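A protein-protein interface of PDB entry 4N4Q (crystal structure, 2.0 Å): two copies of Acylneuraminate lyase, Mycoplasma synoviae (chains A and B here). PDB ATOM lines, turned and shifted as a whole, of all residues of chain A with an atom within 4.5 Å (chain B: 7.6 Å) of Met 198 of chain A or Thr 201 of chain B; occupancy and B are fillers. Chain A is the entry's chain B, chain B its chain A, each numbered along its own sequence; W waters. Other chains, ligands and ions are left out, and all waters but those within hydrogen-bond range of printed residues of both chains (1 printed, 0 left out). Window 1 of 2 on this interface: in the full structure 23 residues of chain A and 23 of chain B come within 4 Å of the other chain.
Leu 173 of chain A touches Met 198 of chain B, and with the chains exchanged Met 198 of chain A touches Leu 173 of chain B. Ala 197 of chain A touches Thr 201 of chain B, and with the chains exchanged Thr 201 of chain A touches Ala 197 of chain B. Met 198 of chain A touches Thr 201 of chain B, but with the chains exchanged Thr 201 of chain A does not touch Met 198 of chain B (4.7 Å). Thr 201 of chain A touches its own counterpart, Thr 201 of chain B. 10 positions are printed for both chains.
Of the printed residues of chain B, Met 198 of chain A touches Leu 173, Met 198 and Thr 201. Of the printed residues of chain A, Thr 201 of chain B touches Ala 197 (3.9 Å), Met 198 (3.7 Å), Thr 201 (2.8 Å) and Met 235 (3.5 Å). Of chain B, only Thr 201 comes within 4 Å of Ala 197 of chain A. No residue of chain B comes within 4 Å of Gly 199 of chain A. Of the printed residues of chain B, Leu 173 of chain A touches Leu 173 (3.2 Å) and Met 198 (3.0 Å). Of the printed residues of chain A, Met 198 of chain B touches Leu 173 (3.0 Å) and Met 198 (3.0 Å). Printed residues of chain A within 4 Å of Gly 203 of chain B: Met 235 (3.5 Å). Trp 226 of chain B touches none of the printed residues of chain A. Phe 190 of chain B touches none of the printed residues of chain A. The nearest printed residue of chain B that does not touch Met 198 of chain A is Met 202 of chain B (4.2 Å).
Of the 11 printed residues of chain A, 5 touch a printed residue of chain B. Printed residues of chain A that touch a printed residue of chain B: Leu 173, Ala 197, Met 198, Thr 201 and Met 235. Hydrophobic or aromatic side chains of chain A that line the printed part of chain B: Leu 173, Ala 197, Met 198 and Met 235. Along chain A the printed residues that touch a printed residue of chain B span positions 173 to 235. Of the 18 printed residues of chain B, 7 touch a printed residue of chain A. Printed residues of chain B that touch a printed residue of chain A: Leu 173, Ala 197, Met 198, Leu 200, Thr 201, Met 202 and Gly 203. Hydrophobic or aromatic side chains of chain B within 4 Å of the printed part of chain A: Leu 173 and Met 198. Along chain B the printed residues that touch a printed residue of chain A span positions 173 to 203. Among the printed residues, no Asp or Glu carboxylate lies within 4 Å of a Lys or Arg side-chain nitrogen of the other chain.
Among the printed residues, pairs that only touch across the chains: Met 198 of chain A with Met 198 of chain B (3.0 Å), Leu 173 of chain A with Met 198 of chain B (3.0 Å), Leu 173 of chain A with Leu 173 of chain B (3.2 Å), Met 235 of chain A with Thr 201 of chain B (3.5 Å), Met 235 of chain A with Gly 203 of chain B (3.5 Å), Met 235 of chain A with Leu 200 of chain B (3.7 Å), Met 198 of chain A with Thr 201 of chain B (3.7 Å), Thr 201 of chain A with Ala 197 of chain B (3.9 Å), Ala 197 of chain A with Thr 201 of chain B (3.9 Å), Met 198 of chain A with Leu 173 of chain B (3.99 Å) and Met 235 of chain A with Met 202 of chain B (3.99 Å).
OG1 of Thr 201 of chain A lies within hydrogen-bond range of O of Ala 197 of chain A (2.7 Å). The backbone carbonyl oxygen (O) of Ala 197 of chain B sits at hydrogen-bond distance from the side-chain hydroxyl (OG1) of Thr 201 of chain B (2.8 Å).
Water W1 lies within hydrogen-bond range of the side-chain hydroxyl of Thr 201 of chain A (2.9 Å), the side-chain hydroxyl of Thr 201 of chain B (3.1 Å) and the indole nitrogen of Trp 226 of chain B (3.3 Å).
The side-chain hydroxyl of Thr 201 of chain A sits at hydrogen-bond distance from the side-chain hydroxyl of Thr 201 of chain B, at 2.8 Å.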
ATOM      1  N   LEU A 173      27.056  14.425   4.891  1.00  0.00           N
ATOM      2  CA  LEU A 173      25.976  15.389   4.763  1.00  0.00           C
ATOM      3  C   LEU A 173      26.315  16.568   3.846  1.00  0.00           C
ATOM      4  O   LEU A 173      25.419  17.302   3.422  1.00  0.00           O
ATOM      5  CB  LEU A 173      25.445  15.794   6.141  1.00  0.00           C
ATOM      6  CG  LEU A 173      24.979  14.520   6.881  1.00  0.00           C
ATOM      7  CD1 LEU A 173      24.731  14.673   8.378  1.00  0.00           C
ATOM      8  CD2 LEU A 173      23.761  13.903   6.194  1.00  0.00           C
ATOM      9  N   ALA A 195      20.680  11.087  11.912  1.00  0.00           N
ATOM     10  CA  ALA A 195      20.857  12.475  11.465  1.00  0.00           C
ATOM     11  C   ALA A 195      19.564  13.002  10.836  1.00  0.00           C
ATOM     12  O   ALA A 195      19.603  13.831   9.917  1.00  0.00           O
ATOM     13  CB  ALA A 195      21.985  12.545  10.419  1.00  0.00           C
ATOM     14  N   LEU A 196      18.424  12.502  11.296  1.00  0.00           N
ATOM     15  CA  LEU A 196      17.136  12.957  10.783  1.00  0.00           C
ATOM     16  C   LEU A 196      17.020  14.505  10.745  1.00  0.00           C
ATOM     17  O   LEU A 196      16.735  15.095   9.682  1.00  0.00           O
ATOM     18  CB  LEU A 196      16.025  12.342  11.634  1.00  0.00           C
ATOM     19  CG  LEU A 196      14.614  12.318  11.042  1.00  0.00           C
ATOM     20  CD1 LEU A 196      13.800  11.233  11.711  1.00  0.00           C
ATOM     21  CD2 LEU A 196      13.930  13.690  11.222  1.00  0.00           C
ATOM     22  N   ALA A 197      17.258  15.156  11.883  1.00  0.00           N
ATOM     23  CA  ALA A 197      17.159  16.639  11.979  1.00  0.00           C
ATOM     24  C   ALA A 197      18.140  17.377  11.066  1.00  0.00           C
ATOM     25  O   ALA A 197      17.802  18.450  10.517  1.00  0.00           O
ATOM     26  CB  ALA A 197      17.330  17.125  13.425  1.00  0.00           C
ATOM     27  N   MET A 198      19.364  16.857  10.958  1.00  0.00           N
ATOM     28  CA  MET A 198      20.326  17.333   9.948  1.00  0.00           C
ATOM     29  C   MET A 198      19.736  17.332   8.533  1.00  0.00           C
ATOM     30  O   MET A 198      19.935  18.276   7.753  1.00  0.00           O
ATOM     31  CB  MET A 198      21.571  16.439   9.912  1.00  0.00           C
ATOM     32  CG  MET A 198      22.155  15.999  11.249  1.00  0.00           C
ATOM     33  SD  MET A 198      23.481  17.045  11.865  1.00  0.00           S
ATOM     34  CE  MET A 198      22.481  18.440  12.311  1.00  0.00           C
ATOM     35  N   GLY A 199      19.090  16.218   8.182  1.00  0.00           N
ATOM     36  CA  GLY A 199      18.440  16.052   6.896  1.00  0.00           C
ATOM     37  C   GLY A 199      17.330  17.072   6.685  1.00  0.00           C
ATOM     38  O   GLY A 199      17.295  17.755   5.652  1.00  0.00           O
ATOM     39  N   LEU A 200      16.436  17.176   7.673  1.00  0.00           N
ATOM     40  CA  LEU A 200      15.367  18.192   7.697  1.00  0.00           C
ATOM     41  C   LEU A 200      15.899  19.591   7.384  1.00  0.00           C
ATOM     42  O   LEU A 200      15.340  20.311   6.532  1.00  0.00           O
ATOM     43  CB  LEU A 200      14.679  18.227   9.076  1.00  0.00           C
ATOM     44  CG  LEU A 200      13.640  17.126   9.349  1.00  0.00           C
ATOM     45  CD1 LEU A 200      13.161  17.218  10.817  1.00  0.00           C
ATOM     46  CD2 LEU A 200      12.468  17.224   8.358  1.00  0.00           C
ATOM     47  N   THR A 201      16.995  19.934   8.060  1.00  0.00           N
ATOM     48  CA  THR A 201      17.646  21.250   7.966  1.00  0.00           C
ATOM     49  C   THR A 201      18.035  21.588   6.531  1.00  0.00           C
ATOM     50  O   THR A 201      17.905  22.739   6.103  1.00  0.00           O
ATOM     51  CB  THR A 201      18.870  21.340   8.921  1.00  0.00           C
ATOM     52  OG1 THR A 201      18.444  21.100  10.267  1.00  0.00           O
ATOM     53  CG2 THR A 201      19.536  22.708   8.878  1.00  0.00           C
ATOM     54  N   MET A 202      18.512  20.588   5.792  1.00  0.00           N
ATOM     55  CA  MET A 202      18.868  20.787   4.386  1.00  0.00           C
ATOM     56  C   MET A 202      17.760  20.448   3.353  1.00  0.00           C
ATOM     57  O   MET A 202      18.024  20.383   2.149  1.00  0.00           O
ATOM     58  CB  MET A 202      20.229  20.157   4.027  1.00  0.00           C
ATOM     59  CG  MET A 202      21.485  21.025   4.301  1.00  0.00           C
ATOM     60  SD  MET A 202      21.304  22.839   4.239  1.00  0.00           S
ATOM     61  CE  MET A 202      21.077  23.145   2.502  1.00  0.00           C
ATOM     62  N   VAL A 234      14.433  19.936  19.355  1.00  0.00           N
ATOM     63  CA  VAL A 234      15.077  19.215  18.237  1.00  0.00           C
ATOM     64  C   VAL A 234      16.348  18.526  18.761  1.00  0.00           C
ATOM     65  O   VAL A 234      16.599  17.342  18.471  1.00  0.00           O
ATOM     66  CB  VAL A 234      15.398  20.138  17.034  1.00  0.00           C
ATOM     67  CG1 VAL A 234      16.264  19.408  15.988  1.00  0.00           C
ATOM     68  CG2 VAL A 234      14.122  20.617  16.389  1.00  0.00           C
ATOM     69  N   MET A 235      17.101  19.263  19.581  1.00  0.00           N
ATOM     70  CA  MET A 235      18.359  18.788  20.157  1.00  0.00           C
ATOM     71  C   MET A 235      18.113  17.672  21.129  1.00  0.00           C
ATOM     72  O   MET A 235      18.652  16.576  20.960  1.00  0.00           O
ATOM     73  CB  MET A 235      19.119  19.930  20.840  1.00  0.00           C
ATOM     74  CG  MET A 235      19.577  20.972  19.851  1.00  0.00           C
ATOM     75  SD  MET A 235      20.202  22.457  20.630  1.00  0.00           S
ATOM     76  CE  MET A 235      19.995  23.621  19.315  1.00  0.00           C
ATOM     77  N   LEU B 173      29.325  14.336  11.877  1.00  0.00           N
ATOM     78  CA  LEU B 173      28.210  14.986  12.579  1.00  0.00           C
ATOM     79  C   LEU B 173      27.551  14.080  13.610  1.00  0.00           C
ATOM     80  O   LEU B 173      26.923  14.564  14.546  1.00  0.00           O
ATOM     81  CB  LEU B 173      27.170  15.550  11.569  1.00  0.00           C
ATOM     82  CG  LEU B 173      27.812  16.578  10.613  1.00  0.00           C
ATOM     83  CD1 LEU B 173      27.156  16.611   9.228  1.00  0.00           C
ATOM     84  CD2 LEU B 173      27.924  17.986  11.219  1.00  0.00           C
ATOM     85  N   PHE B 174      27.689  12.761  13.458  1.00  0.00           N
ATOM     86  CA  PHE B 174      27.176  11.859  14.490  1.00  0.00           C
ATOM     87  C   PHE B 174      27.934  11.964  15.826  1.00  0.00           C
ATOM     88  O   PHE B 174      27.307  12.030  16.895  1.00  0.00           O
ATOM     89  CB  PHE B 174      27.140  10.402  14.018  1.00  0.00           C
ATOM     90  CG  PHE B 174      26.556   9.466  15.029  1.00  0.00           C
ATOM     91  CD1 PHE B 174      25.267   9.682  15.539  1.00  0.00           C
ATOM     92  CD2 PHE B 174      27.287   8.390  15.498  1.00  0.00           C
ATOM     93  CE1 PHE B 174      24.702   8.819  16.480  1.00  0.00           C
ATOM     94  CE2 PHE B 174      26.736   7.516  16.453  1.00  0.00           C
ATOM     95  CZ  PHE B 174      25.438   7.740  16.940  1.00  0.00           C
ATOM     96  N   PHE B 176      29.736  14.440  16.855  1.00  0.00           N
ATOM     97  CA  PHE B 176      29.406  15.778  17.363  1.00  0.00           C
ATOM     98  C   PHE B 176      28.082  15.800  18.120  1.00  0.00           C
ATOM     99  O   PHE B 176      27.972  16.427  19.178  1.00  0.00           O
ATOM    100  CB  PHE B 176      29.328  16.823  16.250  1.00  0.00           C
ATOM    101  CG  PHE B 176      29.080  18.209  16.768  1.00  0.00           C
ATOM    102  CD1 PHE B 176      30.109  18.932  17.383  1.00  0.00           C
ATOM    103  CD2 PHE B 176      27.817  18.771  16.709  1.00  0.00           C
ATOM    104  CE1 PHE B 176      29.884  20.218  17.895  1.00  0.00           C
ATOM    105  CE2 PHE B 176      27.585  20.073  17.206  1.00  0.00           C
ATOM    106  CZ  PHE B 176      28.628  20.790  17.793  1.00  0.00           C
ATOM    107  N   GLU B 177      27.072  15.145  17.565  1.00  0.00           N
ATOM    108  CA  GLU B 177      25.779  15.043  18.259  1.00  0.00           C
ATOM    109  C   GLU B 177      25.982  14.307  19.570  1.00  0.00           C
ATOM    110  O   GLU B 177      25.468  14.720  20.619  1.00  0.00           O
ATOM    111  CB  GLU B 177      24.729  14.367  17.372  1.00  0.00           C
ATOM    112  CG  GLU B 177      23.354  14.153  18.014  1.00  0.00           C
ATOM    113  CD  GLU B 177      23.278  12.884  18.858  1.00  0.00           C
ATOM    114  OE1 GLU B 177      23.805  11.820  18.434  1.00  0.00           O
ATOM    115  OE2 GLU B 177      22.690  12.943  19.961  1.00  0.00           O
ATOM    116  N   PHE B 190      32.522  24.858  16.644  1.00  0.00           N
ATOM    117  CA  PHE B 190      32.276  24.108  15.435  1.00  0.00           C
ATOM    118  C   PHE B 190      33.144  24.605  14.304  1.00  0.00           C
ATOM    119  O   PHE B 190      33.119  25.777  13.935  1.00  0.00           O
ATOM    120  CB  PHE B 190      30.805  24.174  15.054  1.00  0.00           C
ATOM    121  CG  PHE B 190      30.367  23.052  14.165  1.00  0.00           C
ATOM    122  CD1 PHE B 190      30.083  21.795  14.699  1.00  0.00           C
ATOM    123  CD2 PHE B 190      30.212  23.259  12.801  1.00  0.00           C
ATOM    124  CE1 PHE B 190      29.656  20.739  13.867  1.00  0.00           C
ATOM    125  CE2 PHE B 190      29.785  22.235  11.958  1.00  0.00           C
ATOM    126  CZ  PHE B 190      29.501  20.960  12.504  1.00  0.00           C
ATOM    127  N   ALA B 195      29.189  22.911   6.981  1.00  0.00           N
ATOM    128  CA  ALA B 195      28.052  22.348   7.729  1.00  0.00           C
ATOM    129  C   ALA B 195      27.672  23.231   8.911  1.00  0.00           C
ATOM    130  O   ALA B 195      27.221  22.751   9.944  1.00  0.00           O
ATOM    131  CB  ALA B 195      28.362  20.921   8.177  1.00  0.00           C
ATOM    132  N   LEU B 196      27.866  24.545   8.738  1.00  0.00           N
ATOM    133  CA  LEU B 196      27.537  25.534   9.767  1.00  0.00           C
ATOM    134  C   LEU B 196      26.092  25.340  10.268  1.00  0.00           C
ATOM    135  O   LEU B 196      25.847  25.196  11.471  1.00  0.00           O
ATOM    136  CB  LEU B 196      27.732  26.952   9.182  1.00  0.00           C
ATOM    137  CG  LEU B 196      27.754  28.190  10.097  1.00  0.00           C
ATOM    138  CD1 LEU B 196      28.249  29.423   9.346  1.00  0.00           C
ATOM    139  CD2 LEU B 196      26.402  28.488  10.682  1.00  0.00           C
ATOM    140  N   ALA B 197      25.137  25.316   9.338  1.00  0.00           N
ATOM    141  CA  ALA B 197      23.724  25.177   9.720  1.00  0.00           C
ATOM    142  C   ALA B 197      23.438  23.817  10.372  1.00  0.00           C
ATOM    143  O   ALA B 197      22.552  23.682  11.207  1.00  0.00           O
ATOM    144  CB  ALA B 197      22.825  25.409   8.541  1.00  0.00           C
ATOM    145  N   MET B 198      24.206  22.804  10.018  1.00  0.00           N
ATOM    146  CA  MET B 198      24.007  21.536  10.695  1.00  0.00           C
ATOM    147  C   MET B 198      24.579  21.529  12.106  1.00  0.00           C
ATOM    148  O   MET B 198      24.037  20.875  13.010  1.00  0.00           O
ATOM    149  CB  MET B 198      24.493  20.399   9.827  1.00  0.00           C
ATOM    150  CG  MET B 198      23.432  20.167   8.765  1.00  0.00           C
ATOM    151  SD  MET B 198      24.063  19.141   7.515  1.00  0.00           S
ATOM    152  CE  MET B 198      24.274  17.656   8.462  1.00  0.00           C
ATOM    153  N   GLY B 199      25.633  22.310  12.311  1.00  0.00           N
ATOM    154  CA  GLY B 199      26.168  22.493  13.652  1.00  0.00           C
ATOM    155  C   GLY B 199      25.193  23.263  14.515  1.00  0.00           C
ATOM    156  O   GLY B 199      25.023  22.961  15.713  1.00  0.00           O
ATOM    157  N   LEU B 200      24.574  24.279  13.919  1.00  0.00           N
ATOM    158  CA  LEU B 200      23.534  25.054  14.598  1.00  0.00           C
ATOM    159  C   LEU B 200      22.417  24.113  15.054  1.00  0.00           C
ATOM    160  O   LEU B 200      22.058  24.103  16.242  1.00  0.00           O
ATOM    161  CB  LEU B 200      22.978  26.125  13.678  1.00  0.00           C
ATOM    162  CG  LEU B 200      23.820  27.387  13.459  1.00  0.00           C
ATOM    163  CD1 LEU B 200      23.259  28.178  12.263  1.00  0.00           C
ATOM    164  CD2 LEU B 200      23.836  28.258  14.728  1.00  0.00           C
ATOM    165  N   THR B 201      21.936  23.271  14.127  1.00  0.00           N
ATOM    166  CA  THR B 201      20.805  22.365  14.408  1.00  0.00           C
ATOM    167  C   THR B 201      21.030  21.548  15.681  1.00  0.00           C
ATOM    168  O   THR B 201      20.084  21.328  16.430  1.00  0.00           O
ATOM    169  CB  THR B 201      20.444  21.437  13.218  1.00  0.00           C
ATOM    170  OG1 THR B 201      20.296  22.206  12.021  1.00  0.00           O
ATOM    171  CG2 THR B 201      19.125  20.689  13.483  1.00  0.00           C
ATOM    172  N   MET B 202      22.281  21.134  15.928  1.00  0.00           N
ATOM    173  CA  MET B 202      22.645  20.330  17.104  1.00  0.00           C
ATOM    174  C   MET B 202      23.236  21.133  18.260  1.00  0.00           C
ATOM    175  O   MET B 202      23.734  20.553  19.256  1.00  0.00           O
ATOM    176  CB  MET B 202      23.607  19.186  16.720  1.00  0.00           C
ATOM    177  CG  MET B 202      23.449  17.926  17.568  1.00  0.00           C
ATOM    178  SD  MET B 202      21.724  17.403  17.826  1.00  0.00           S
ATOM    179  CE  MET B 202      21.043  17.418  16.156  1.00  0.00           C
ATOM    180  N   GLY B 203      23.180  22.458  18.141  1.00  0.00           N
ATOM    181  CA  GLY B 203      23.517  23.320  19.271  1.00  0.00           C
ATOM    182  C   GLY B 203      24.842  24.065  19.275  1.00  0.00           C
ATOM    183  O   GLY B 203      25.177  24.687  20.282  1.00  0.00           O
ATOM    184  N   ALA B 204      25.609  23.998  18.189  1.00  0.00           N
ATOM    185  CA  ALA B 204      26.832  24.814  18.080  1.00  0.00           C
ATOM    186  C   ALA B 204      26.445  26.295  18.092  1.00  0.00           C
ATOM    187  O   ALA B 204      25.434  26.673  17.504  1.00  0.00           O
ATOM    188  CB  ALA B 204      27.598  24.484  16.821  1.00  0.00           C
ATOM    189  N   PHE B 207      31.681  29.383  15.956  1.00  0.00           N
ATOM    190  CA  PHE B 207      32.189  28.808  14.719  1.00  0.00           C
ATOM    191  C   PHE B 207      33.583  29.339  14.407  1.00  0.00           C
ATOM    192  O   PHE B 207      33.798  30.549  14.361  1.00  0.00           O
ATOM    193  CB  PHE B 207      31.180  29.068  13.591  1.00  0.00           C
ATOM    194  CG  PHE B 207      29.820  28.435  13.859  1.00  0.00           C
ATOM    195  CD1 PHE B 207      28.833  29.125  14.568  1.00  0.00           C
ATOM    196  CD2 PHE B 207      29.556  27.130  13.455  1.00  0.00           C
ATOM    197  CE1 PHE B 207      27.584  28.534  14.841  1.00  0.00           C
ATOM    198  CE2 PHE B 207      28.323  26.532  13.714  1.00  0.00           C
ATOM    199  CZ  PHE B 207      27.331  27.236  14.409  1.00  0.00           C
ATOM    200  N   TRP B 226      18.626  31.238  10.602  1.00  0.00           N
ATOM    201  CA  TRP B 226      18.373  30.092  11.458  1.00  0.00           C
ATOM    202  C   TRP B 226      17.626  30.507  12.708  1.00  0.00           C
ATOM    203  O   TRP B 226      16.591  29.919  13.031  1.00  0.00           O
ATOM    204  CB  TRP B 226      19.670  29.376  11.842  1.00  0.00           C
ATOM    205  CG  TRP B 226      19.461  28.085  12.583  1.00  0.00           C
ATOM    206  CD1 TRP B 226      19.208  26.856  12.028  1.00  0.00           C
ATOM    207  CD2 TRP B 226      19.504  27.878  14.006  1.00  0.00           C
ATOM    208  NE1 TRP B 226      19.097  25.915  13.007  1.00  0.00           N
ATOM    209  CE2 TRP B 226      19.274  26.506  14.230  1.00  0.00           C
ATOM    210  CE3 TRP B 226      19.713  28.719  15.110  1.00  0.00           C
ATOM    211  CZ2 TRP B 226      19.246  25.949  15.511  1.00  0.00           C
ATOM    212  CZ3 TRP B 226      19.681  28.174  16.380  1.00  0.00           C
ATOM    213  CH2 TRP B 226      19.454  26.792  16.575  1.00  0.00           C
ATOM    214  N   VAL B 234      17.717  29.336   5.214  1.00  0.00           N
ATOM    215  CA  VAL B 234      18.820  28.560   5.801  1.00  0.00           C
ATOM    216  C   VAL B 234      19.391  27.629   4.725  1.00  0.00           C
ATOM    217  O   VAL B 234      20.613  27.514   4.567  1.00  0.00           O
ATOM    218  CB  VAL B 234      18.410  27.760   7.080  1.00  0.00           C
ATOM    219  CG1 VAL B 234      19.548  26.847   7.547  1.00  0.00           C
ATOM    220  CG2 VAL B 234      18.005  28.693   8.210  1.00  0.00           C
HETATM  221  O   HOH W   1      17.425  23.362  11.773  1.00  0.00           O
